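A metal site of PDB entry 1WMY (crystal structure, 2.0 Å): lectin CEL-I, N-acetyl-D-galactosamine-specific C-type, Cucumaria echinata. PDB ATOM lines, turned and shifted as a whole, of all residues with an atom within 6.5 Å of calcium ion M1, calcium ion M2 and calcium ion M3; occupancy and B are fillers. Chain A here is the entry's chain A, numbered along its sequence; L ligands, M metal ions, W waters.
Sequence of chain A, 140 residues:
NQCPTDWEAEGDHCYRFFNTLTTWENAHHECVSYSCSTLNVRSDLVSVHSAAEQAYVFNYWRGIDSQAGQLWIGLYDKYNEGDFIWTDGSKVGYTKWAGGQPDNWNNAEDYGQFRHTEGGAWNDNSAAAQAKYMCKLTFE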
ATOM      1  N   ASP A  77       2.541 -10.317   2.732  1.00  0.00           N
ATOM      2  CA  ASP A  77       3.708 -11.094   3.142  1.00  0.00           C
ATOM      3  C   ASP A  77       3.984 -11.012   4.667  1.00  0.00           C
ATOM      4  O   ASP A  77       5.158 -10.992   5.119  1.00  0.00           O
ATOM      5  CB  ASP A  77       4.930 -10.677   2.346  1.00  0.00           C
ATOM      6  CG  ASP A  77       5.514  -9.354   2.803  1.00  0.00           C
ATOM      7  OD1 ASP A  77       4.807  -8.495   3.349  1.00  0.00           O
ATOM      8  OD2 ASP A  77       6.717  -9.066   2.617  1.00  0.00           O
ATOM      9  N   LYS A  78       2.915 -11.004   5.414  1.00  0.00           N
ATOM     10  CA  LYS A  78       2.952 -11.077   6.857  1.00  0.00           C
ATOM     11  C   LYS A  78       3.663 -12.323   7.372  1.00  0.00           C
ATOM     12  O   LYS A  78       4.430 -12.229   8.354  1.00  0.00           O
ATOM     13  CB  LYS A  78       1.487 -10.964   7.373  1.00  0.00           C
ATOM     14  CG  LYS A  78       1.248 -10.878   8.846  1.00  0.00           C
ATOM     15  CD  LYS A  78      -0.054 -10.035   9.209  1.00  0.00           C
ATOM     16  CE  LYS A  78      -1.359 -10.658   8.579  1.00  0.00           C
ATOM     17  NZ  LYS A  78      -2.719 -10.012   8.961  1.00  0.00           N
ATOM     18  N   ASN A  80       5.678 -14.587   5.743  1.00  0.00           N
ATOM     19  CA  ASN A  80       6.988 -14.775   5.185  1.00  0.00           C
ATOM     20  C   ASN A  80       7.373 -13.503   4.422  1.00  0.00           C
ATOM     21  O   ASN A  80       7.052 -13.342   3.268  1.00  0.00           O
ATOM     22  CB  ASN A  80       6.952 -15.981   4.253  1.00  0.00           C
ATOM     23  CG  ASN A  80       6.859 -17.307   4.988  1.00  0.00           C
ATOM     24  OD1 ASN A  80       7.879 -17.890   5.359  1.00  0.00           O
ATOM     25  ND2 ASN A  80       5.641 -17.721   5.293  1.00  0.00           N
ATOM     26  N   GLU A  81       8.159 -12.645   5.056  1.00  0.00           N
ATOM     27  CA  GLU A  81       8.520 -11.379   4.527  1.00  0.00           C
ATOM     28  C   GLU A  81       9.189 -11.573   3.177  1.00  0.00           C
ATOM     29  O   GLU A  81      10.050 -12.426   3.098  1.00  0.00           O
ATOM     30  CB  GLU A  81       9.452 -10.655   5.529  1.00  0.00           C
ATOM     31  CG  GLU A  81      10.028  -9.337   4.966  1.00  0.00           C
ATOM     32  CD  GLU A  81       8.939  -8.323   4.608  1.00  0.00           C
ATOM     33  OE1 GLU A  81       8.991  -7.687   3.527  1.00  0.00           O
ATOM     34  OE2 GLU A  81       8.007  -8.131   5.381  1.00  0.00           O
ATOM     35  N   GLY A  82       8.781 -10.826   2.164  1.00  0.00           N
ATOM     36  CA  GLY A  82       9.319 -10.880   0.796  1.00  0.00           C
ATOM     37  C   GLY A  82       8.674 -11.945  -0.096  1.00  0.00           C
ATOM     38  O   GLY A  82       8.918 -11.953  -1.256  1.00  0.00           O
ATOM     39  N   PHE A  84       5.199 -12.900  -1.036  1.00  0.00           N
ATOM     40  CA  PHE A  84       3.790 -12.520  -1.047  1.00  0.00           C
ATOM     41  C   PHE A  84       2.917 -13.701  -1.490  1.00  0.00           C
ATOM     42  O   PHE A  84       3.308 -14.473  -2.409  1.00  0.00           O
ATOM     43  CB  PHE A  84       3.617 -11.337  -1.968  1.00  0.00           C
ATOM     44  CG  PHE A  84       4.093 -10.051  -1.370  1.00  0.00           C
ATOM     45  CD1 PHE A  84       3.220  -9.263  -0.678  1.00  0.00           C
ATOM     46  CD2 PHE A  84       5.412  -9.665  -1.494  1.00  0.00           C
ATOM     47  CE1 PHE A  84       3.634  -8.052  -0.114  1.00  0.00           C
ATOM     48  CE2 PHE A  84       5.859  -8.491  -0.926  1.00  0.00           C
ATOM     49  CZ  PHE A  84       4.952  -7.669  -0.248  1.00  0.00           C
ATOM     50  N   GLY A 100      10.715  -0.228  -7.988  1.00  0.00           N
ATOM     51  CA  GLY A 100      11.190  -0.029  -6.647  1.00  0.00           C
ATOM     52  C   GLY A 100      10.334  -0.702  -5.597  1.00  0.00           C
ATOM     53  O   GLY A 100      10.490  -0.463  -4.398  1.00  0.00           O
ATOM     54  N   GLN A 101       9.387  -1.514  -6.073  1.00  0.00           N
ATOM     55  CA  GLN A 101       8.503  -2.289  -5.169  1.00  0.00           C
ATOM     56  C   GLN A 101       8.644  -3.812  -5.397  1.00  0.00           C
ATOM     57  O   GLN A 101       8.951  -4.229  -6.480  1.00  0.00           O
ATOM     58  CB  GLN A 101       7.079  -1.850  -5.392  1.00  0.00           C
ATOM     59  CG  GLN A 101       6.806  -0.341  -5.298  1.00  0.00           C
ATOM     60  CD  GLN A 101       7.167   0.237  -3.977  1.00  0.00           C
ATOM     61  OE1 GLN A 101       7.059  -0.458  -2.945  1.00  0.00           O
ATOM     62  NE2 GLN A 101       7.631   1.520  -3.972  1.00  0.00           N
ATOM     63  N   PRO A 102       8.346  -4.644  -4.396  1.00  0.00           N
ATOM     64  CA  PRO A 102       7.928  -4.247  -3.062  1.00  0.00           C
ATOM     65  C   PRO A 102       9.162  -3.913  -2.200  1.00  0.00           C
ATOM     66  O   PRO A 102      10.133  -4.678  -2.255  1.00  0.00           O
ATOM     67  CB  PRO A 102       7.187  -5.490  -2.558  1.00  0.00           C
ATOM     68  CG  PRO A 102       7.832  -6.661  -3.211  1.00  0.00           C
ATOM     69  CD  PRO A 102       8.364  -6.120  -4.556  1.00  0.00           C
ATOM     70  N   ASP A 103       9.142  -2.811  -1.462  1.00  0.00           N
ATOM     71  CA  ASP A 103      10.359  -2.357  -0.734  1.00  0.00           C
ATOM     72  C   ASP A 103      10.219  -2.487   0.792  1.00  0.00           C
ATOM     73  O   ASP A 103      11.175  -2.284   1.519  1.00  0.00           O
ATOM     74  CB  ASP A 103      10.708  -0.948  -1.099  1.00  0.00           C
ATOM     75  CG  ASP A 103       9.574   0.052  -0.707  1.00  0.00           C
ATOM     76  OD1 ASP A 103       9.742   1.279  -0.864  1.00  0.00           O
ATOM     77  OD2 ASP A 103       8.507  -0.343  -0.210  1.00  0.00           O
ATOM     78  N   ASN A 104       9.074  -2.939   1.294  1.00  0.00           N
ATOM     79  CA  ASN A 104       8.909  -3.160   2.753  1.00  0.00           C
ATOM     80  C   ASN A 104       9.324  -1.906   3.534  1.00  0.00           C
ATOM     81  O   ASN A 104      10.139  -1.974   4.510  1.00  0.00           O
ATOM     82  CB  ASN A 104       9.756  -4.357   3.256  1.00  0.00           C
ATOM     83  CG  ASN A 104       9.214  -4.898   4.603  1.00  0.00           C
ATOM     84  OD1 ASN A 104       8.033  -4.951   4.808  1.00  0.00           O
ATOM     85  ND2 ASN A 104      10.127  -5.248   5.533  1.00  0.00           N
ATOM     86  N   TRP A 105       8.893  -0.757   3.025  1.00  0.00           N
ATOM     87  CA  TRP A 105       9.369   0.534   3.559  1.00  0.00           C
ATOM     88  C   TRP A 105       9.226   0.650   5.073  1.00  0.00           C
ATOM     89  O   TRP A 105       8.200   0.278   5.651  1.00  0.00           O
ATOM     90  CB  TRP A 105       8.643   1.703   2.857  1.00  0.00           C
ATOM     91  CG  TRP A 105       9.100   2.976   3.325  1.00  0.00           C
ATOM     92  CD1 TRP A 105      10.261   3.604   2.983  1.00  0.00           C
ATOM     93  CD2 TRP A 105       8.498   3.782   4.328  1.00  0.00           C
ATOM     94  NE1 TRP A 105      10.391   4.777   3.660  1.00  0.00           N
ATOM     95  CE2 TRP A 105       9.333   4.916   4.517  1.00  0.00           C
ATOM     96  CE3 TRP A 105       7.337   3.674   5.098  1.00  0.00           C
ATOM     97  CZ2 TRP A 105       9.014   5.955   5.398  1.00  0.00           C
ATOM     98  CZ3 TRP A 105       7.045   4.704   6.019  1.00  0.00           C
ATOM     99  CH2 TRP A 105       7.884   5.817   6.161  1.00  0.00           C
ATOM    100  N   ASN A 107      10.556  -1.158   7.231  1.00  0.00           N
ATOM    101  CA  ASN A 107      10.402  -2.515   7.691  1.00  0.00           C
ATOM    102  C   ASN A 107       8.951  -2.833   8.098  1.00  0.00           C
ATOM    103  O   ASN A 107       8.692  -3.688   8.953  1.00  0.00           O
ATOM    104  CB  ASN A 107      11.447  -2.856   8.819  1.00  0.00           C
ATOM    105  CG  ASN A 107      11.716  -4.426   8.940  1.00  0.00           C
ATOM    106  OD1 ASN A 107      11.442  -5.196   7.981  1.00  0.00           O
ATOM    107  ND2 ASN A 107      12.208  -4.887  10.117  1.00  0.00           N
ATOM    108  N   ALA A 108       7.977  -2.167   7.459  1.00  0.00           N
ATOM    109  CA  ALA A 108       6.621  -2.239   7.903  1.00  0.00           C
ATOM    110  C   ALA A 108       5.524  -2.246   6.852  1.00  0.00           C
ATOM    111  O   ALA A 108       4.431  -1.741   7.149  1.00  0.00           O
ATOM    112  CB  ALA A 108       6.315  -1.066   8.904  1.00  0.00           C
ATOM    113  N   GLU A 109       5.790  -2.775   5.669  1.00  0.00           N
ATOM    114  CA  GLU A 109       4.790  -2.873   4.628  1.00  0.00           C
ATOM    115  C   GLU A 109       4.554  -4.304   4.159  1.00  0.00           C
ATOM    116  O   GLU A 109       5.370  -4.868   3.427  1.00  0.00           O
ATOM    117  CB  GLU A 109       5.205  -1.989   3.419  1.00  0.00           C
ATOM    118  CG  GLU A 109       5.406  -0.510   3.807  1.00  0.00           C
ATOM    119  CD  GLU A 109       5.542   0.395   2.571  1.00  0.00           C
ATOM    120  OE1 GLU A 109       6.230  -0.013   1.597  1.00  0.00           O
ATOM    121  OE2 GLU A 109       4.913   1.486   2.523  1.00  0.00           O
ATOM    122  N   ASP A 110       3.411  -4.882   4.568  1.00  0.00           N
ATOM    123  CA  ASP A 110       3.131  -6.254   4.226  1.00  0.00           C
ATOM    124  C   ASP A 110       1.893  -6.444   3.317  1.00  0.00           C
ATOM    125  O   ASP A 110       1.399  -7.535   3.182  1.00  0.00           O
ATOM    126  CB  ASP A 110       3.050  -7.102   5.503  1.00  0.00           C
ATOM    127  CG  ASP A 110       4.402  -7.222   6.205  1.00  0.00           C
ATOM    128  OD1 ASP A 110       4.417  -7.757   7.292  1.00  0.00           O
ATOM    129  OD2 ASP A 110       5.507  -6.873   5.673  1.00  0.00           O
ATOM    130  N   TYR A 111       1.395  -5.369   2.742  1.00  0.00           N
ATOM    131  CA  TYR A 111       0.046  -5.427   2.200  1.00  0.00           C
ATOM    132  C   TYR A 111       0.011  -4.779   0.826  1.00  0.00           C
ATOM    133  O   TYR A 111       0.381  -3.612   0.645  1.00  0.00           O
ATOM    134  CB  TYR A 111      -0.946  -4.696   3.081  1.00  0.00           C
ATOM    135  CG  TYR A 111      -0.941  -5.178   4.511  1.00  0.00           C
ATOM    136  CD1 TYR A 111      -0.568  -4.353   5.536  1.00  0.00           C
ATOM    137  CD2 TYR A 111      -1.359  -6.467   4.803  1.00  0.00           C
ATOM    138  CE1 TYR A 111      -0.575  -4.807   6.834  1.00  0.00           C
ATOM    139  CE2 TYR A 111      -1.351  -6.963   6.048  1.00  0.00           C
ATOM    140  CZ  TYR A 111      -0.994  -6.144   7.098  1.00  0.00           C
ATOM    141  OH  TYR A 111      -1.020  -6.642   8.390  1.00  0.00           O
ATOM    142  N   ARG A 115      -1.725   1.061  -7.357  1.00  0.00           N
ATOM    143  CA  ARG A 115      -1.769   2.511  -7.500  1.00  0.00           C
ATOM    144  C   ARG A 115      -2.807   2.886  -8.575  1.00  0.00           C
ATOM    145  O   ARG A 115      -3.135   2.053  -9.437  1.00  0.00           O
ATOM    146  CB  ARG A 115      -0.405   2.994  -7.958  1.00  0.00           C
ATOM    147  CG  ARG A 115       0.672   2.814  -6.897  1.00  0.00           C
ATOM    148  CD  ARG A 115       1.929   3.428  -7.416  1.00  0.00           C
ATOM    149  NE  ARG A 115       3.016   3.215  -6.494  1.00  0.00           N
ATOM    150  CZ  ARG A 115       4.280   3.436  -6.765  1.00  0.00           C
ATOM    151  NH1 ARG A 115       4.654   3.912  -7.977  1.00  0.00           N
ATOM    152  NH2 ARG A 115       5.174   3.175  -5.803  1.00  0.00           N
ATOM    153  N   ASN A 123       1.999  -1.650  -5.276  1.00  0.00           N
ATOM    154  CA  ASN A 123       2.874  -1.205  -4.214  1.00  0.00           C
ATOM    155  C   ASN A 123       2.534  -2.030  -2.958  1.00  0.00           C
ATOM    156  O   ASN A 123       1.417  -2.537  -2.811  1.00  0.00           O
ATOM    157  CB  ASN A 123       2.580   0.252  -3.946  1.00  0.00           C
ATOM    158  CG  ASN A 123       3.331   0.773  -2.740  1.00  0.00           C
ATOM    159  OD1 ASN A 123       4.516   0.555  -2.624  1.00  0.00           O
ATOM    160  ND2 ASN A 123       2.650   1.495  -1.881  1.00  0.00           N
ATOM    161  N   ASP A 124       3.523  -2.221  -2.080  1.00  0.00           N
ATOM    162  CA  ASP A 124       3.260  -2.731  -0.751  1.00  0.00           C
ATOM    163  C   ASP A 124       3.147  -1.544   0.197  1.00  0.00           C
ATOM    164  O   ASP A 124       3.919  -0.595   0.120  1.00  0.00           O
ATOM    165  CB  ASP A 124       4.314  -3.701  -0.284  1.00  0.00           C
ATOM    166  CG  ASP A 124       5.738  -3.113  -0.257  1.00  0.00           C
ATOM    167  OD1 ASP A 124       5.982  -2.081  -0.895  1.00  0.00           O
ATOM    168  OD2 ASP A 124       6.638  -3.690   0.390  1.00  0.00           O
ATOM    169  N   ASN A 125       2.216  -1.650   1.142  1.00  0.00           N
ATOM    170  CA  ASN A 125       1.984  -0.583   2.065  1.00  0.00           C
ATOM    171  C   ASN A 125       1.694  -1.163   3.458  1.00  0.00           C
ATOM    172  O   ASN A 125       1.708  -2.369   3.678  1.00  0.00           O
ATOM    173  CB  ASN A 125       0.862   0.288   1.519  1.00  0.00           C
ATOM    174  CG  ASN A 125       0.966   1.756   1.935  1.00  0.00           C
ATOM    175  OD1 ASN A 125       1.339   2.088   3.058  1.00  0.00           O
ATOM    176  ND2 ASN A 125       0.511   2.612   1.047  1.00  0.00           N
HETATM  177  C1  LIG L   1       5.235   4.379   1.356  1.00  0.00           C
HETATM  178  C2  LIG L   1       4.912   3.779   0.014  1.00  0.00           C
HETATM  179  O1  LIG L   1       4.869   2.322   0.119  1.00  0.00           O
HETATM  180  C3  LIG L   1       3.549   4.364  -0.349  1.00  0.00           C
HETATM  181  C4  LIG L   1       5.968   4.132  -1.023  1.00  0.00           C
HETATM  182  C5  LIG L   1       7.322   3.553  -0.712  1.00  0.00           C
HETATM  183  O2  LIG L   1       7.499   2.280  -1.282  1.00  0.00           O
HETATM  184  C6  LIG L   1       8.438   4.429  -1.206  1.00  0.00           C
HETATM  185 CA    CA M   1       6.123   0.254  -0.743  1.00  0.00          CA
HETATM  186 CA    CA M   2       6.696  -6.866   3.695  1.00  0.00          CA
HETATM  187 CA    CA M   3       6.855  -7.927   7.403  1.00  0.00          CA
HETATM  188  O   HOH W   1       6.611 -10.169   7.209  1.00  0.00           O
HETATM  189  O   HOH W   2       7.391  -5.667   7.529  1.00  0.00           O
HETATM  190  O   HOH W   3       6.469  -8.246   9.754  1.00  0.00           O
HETATM  191  O   HOH W   4       7.409  -5.968   1.479  1.00  0.00           O
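Calcium ion M2 is bound by OD2 of Asp 110, O of Glu 109, OE1 of Glu 81, OD2 of Asp 77, OE2 of Glu 81, water W4, OD1 of Asp 77 and OD1 of Asn 104. Calcium ion M2 has eight donor atoms within binding distance.
Water W4 bridges the side-chain carboxylate (OD2) of Asp 124 and the backbone NH (N) of Asn 104. Water W2 lies within hydrogen-bond range of O of Asn 107 (2.8 Å) and ND2 of Asn 104 (3.4 Å).
Along chain A the residues within 4 Å of calcium ion M1 span positions 101 to 124.
Five residues have an atom within 4 Å of calcium ion M2: Asp 77, Glu 81, Asn 104, Glu 109 and Asp 110. The nearest printed residue that does not touch calcium ion M2 is Phe 84 (4.4 Å).
The backbone NH (N) of Trp 105 sits close to the side-chain carboxylate (OD2) of Asp 103 (3.3 Å). N of Asn 104 lies within hydrogen-bond range of OD2 of Asp 124 (2.7 Å). OE1 of Glu 109 lies close to N of Trp 105. OD2 of Asp 77 sits close to N of Gly 82 (2.8 Å). ND2 of Asn 104 lies within hydrogen-bond range of OD1 of Asn 107, 2.8 Å away. The guanidinium group (NH2) of Arg 115 sits close to the side-chain amide nitrogen (NE2) of Gln 101, 3.5 Å away. The backbone carbonyl oxygen (O) of Asn 125 is in hydrogen-bond range of the backbone NH (N) of Asp 110, 3.2 Å away.
Calcium ion M1 is bound by OD1 of Asp 124 (2.3 Å), OE1 of Glu 109 (2.4 Å), OD1 of Asn 123 (2.5 Å), OE1 of Gln 101 (2.5 Å), O2 of the ligand (2.5 Å), OD2 of Asp 103 (2.5 Å), O of Asp 124 (2.5 Å) and O1 of the ligand (2.6 Å).
Within 4 Å of calcium ion M3: Glu 81 and Asp 110.
Calcium ion M3 is bound by water W1 (2.3 Å), water W2 (2.3 Å), OE2 of Glu 81 (2.3 Å), water W3 (2.4 Å), OD2 of Asp 110 (2.4 Å) and OD1 of Asp 110 (2.4 Å).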
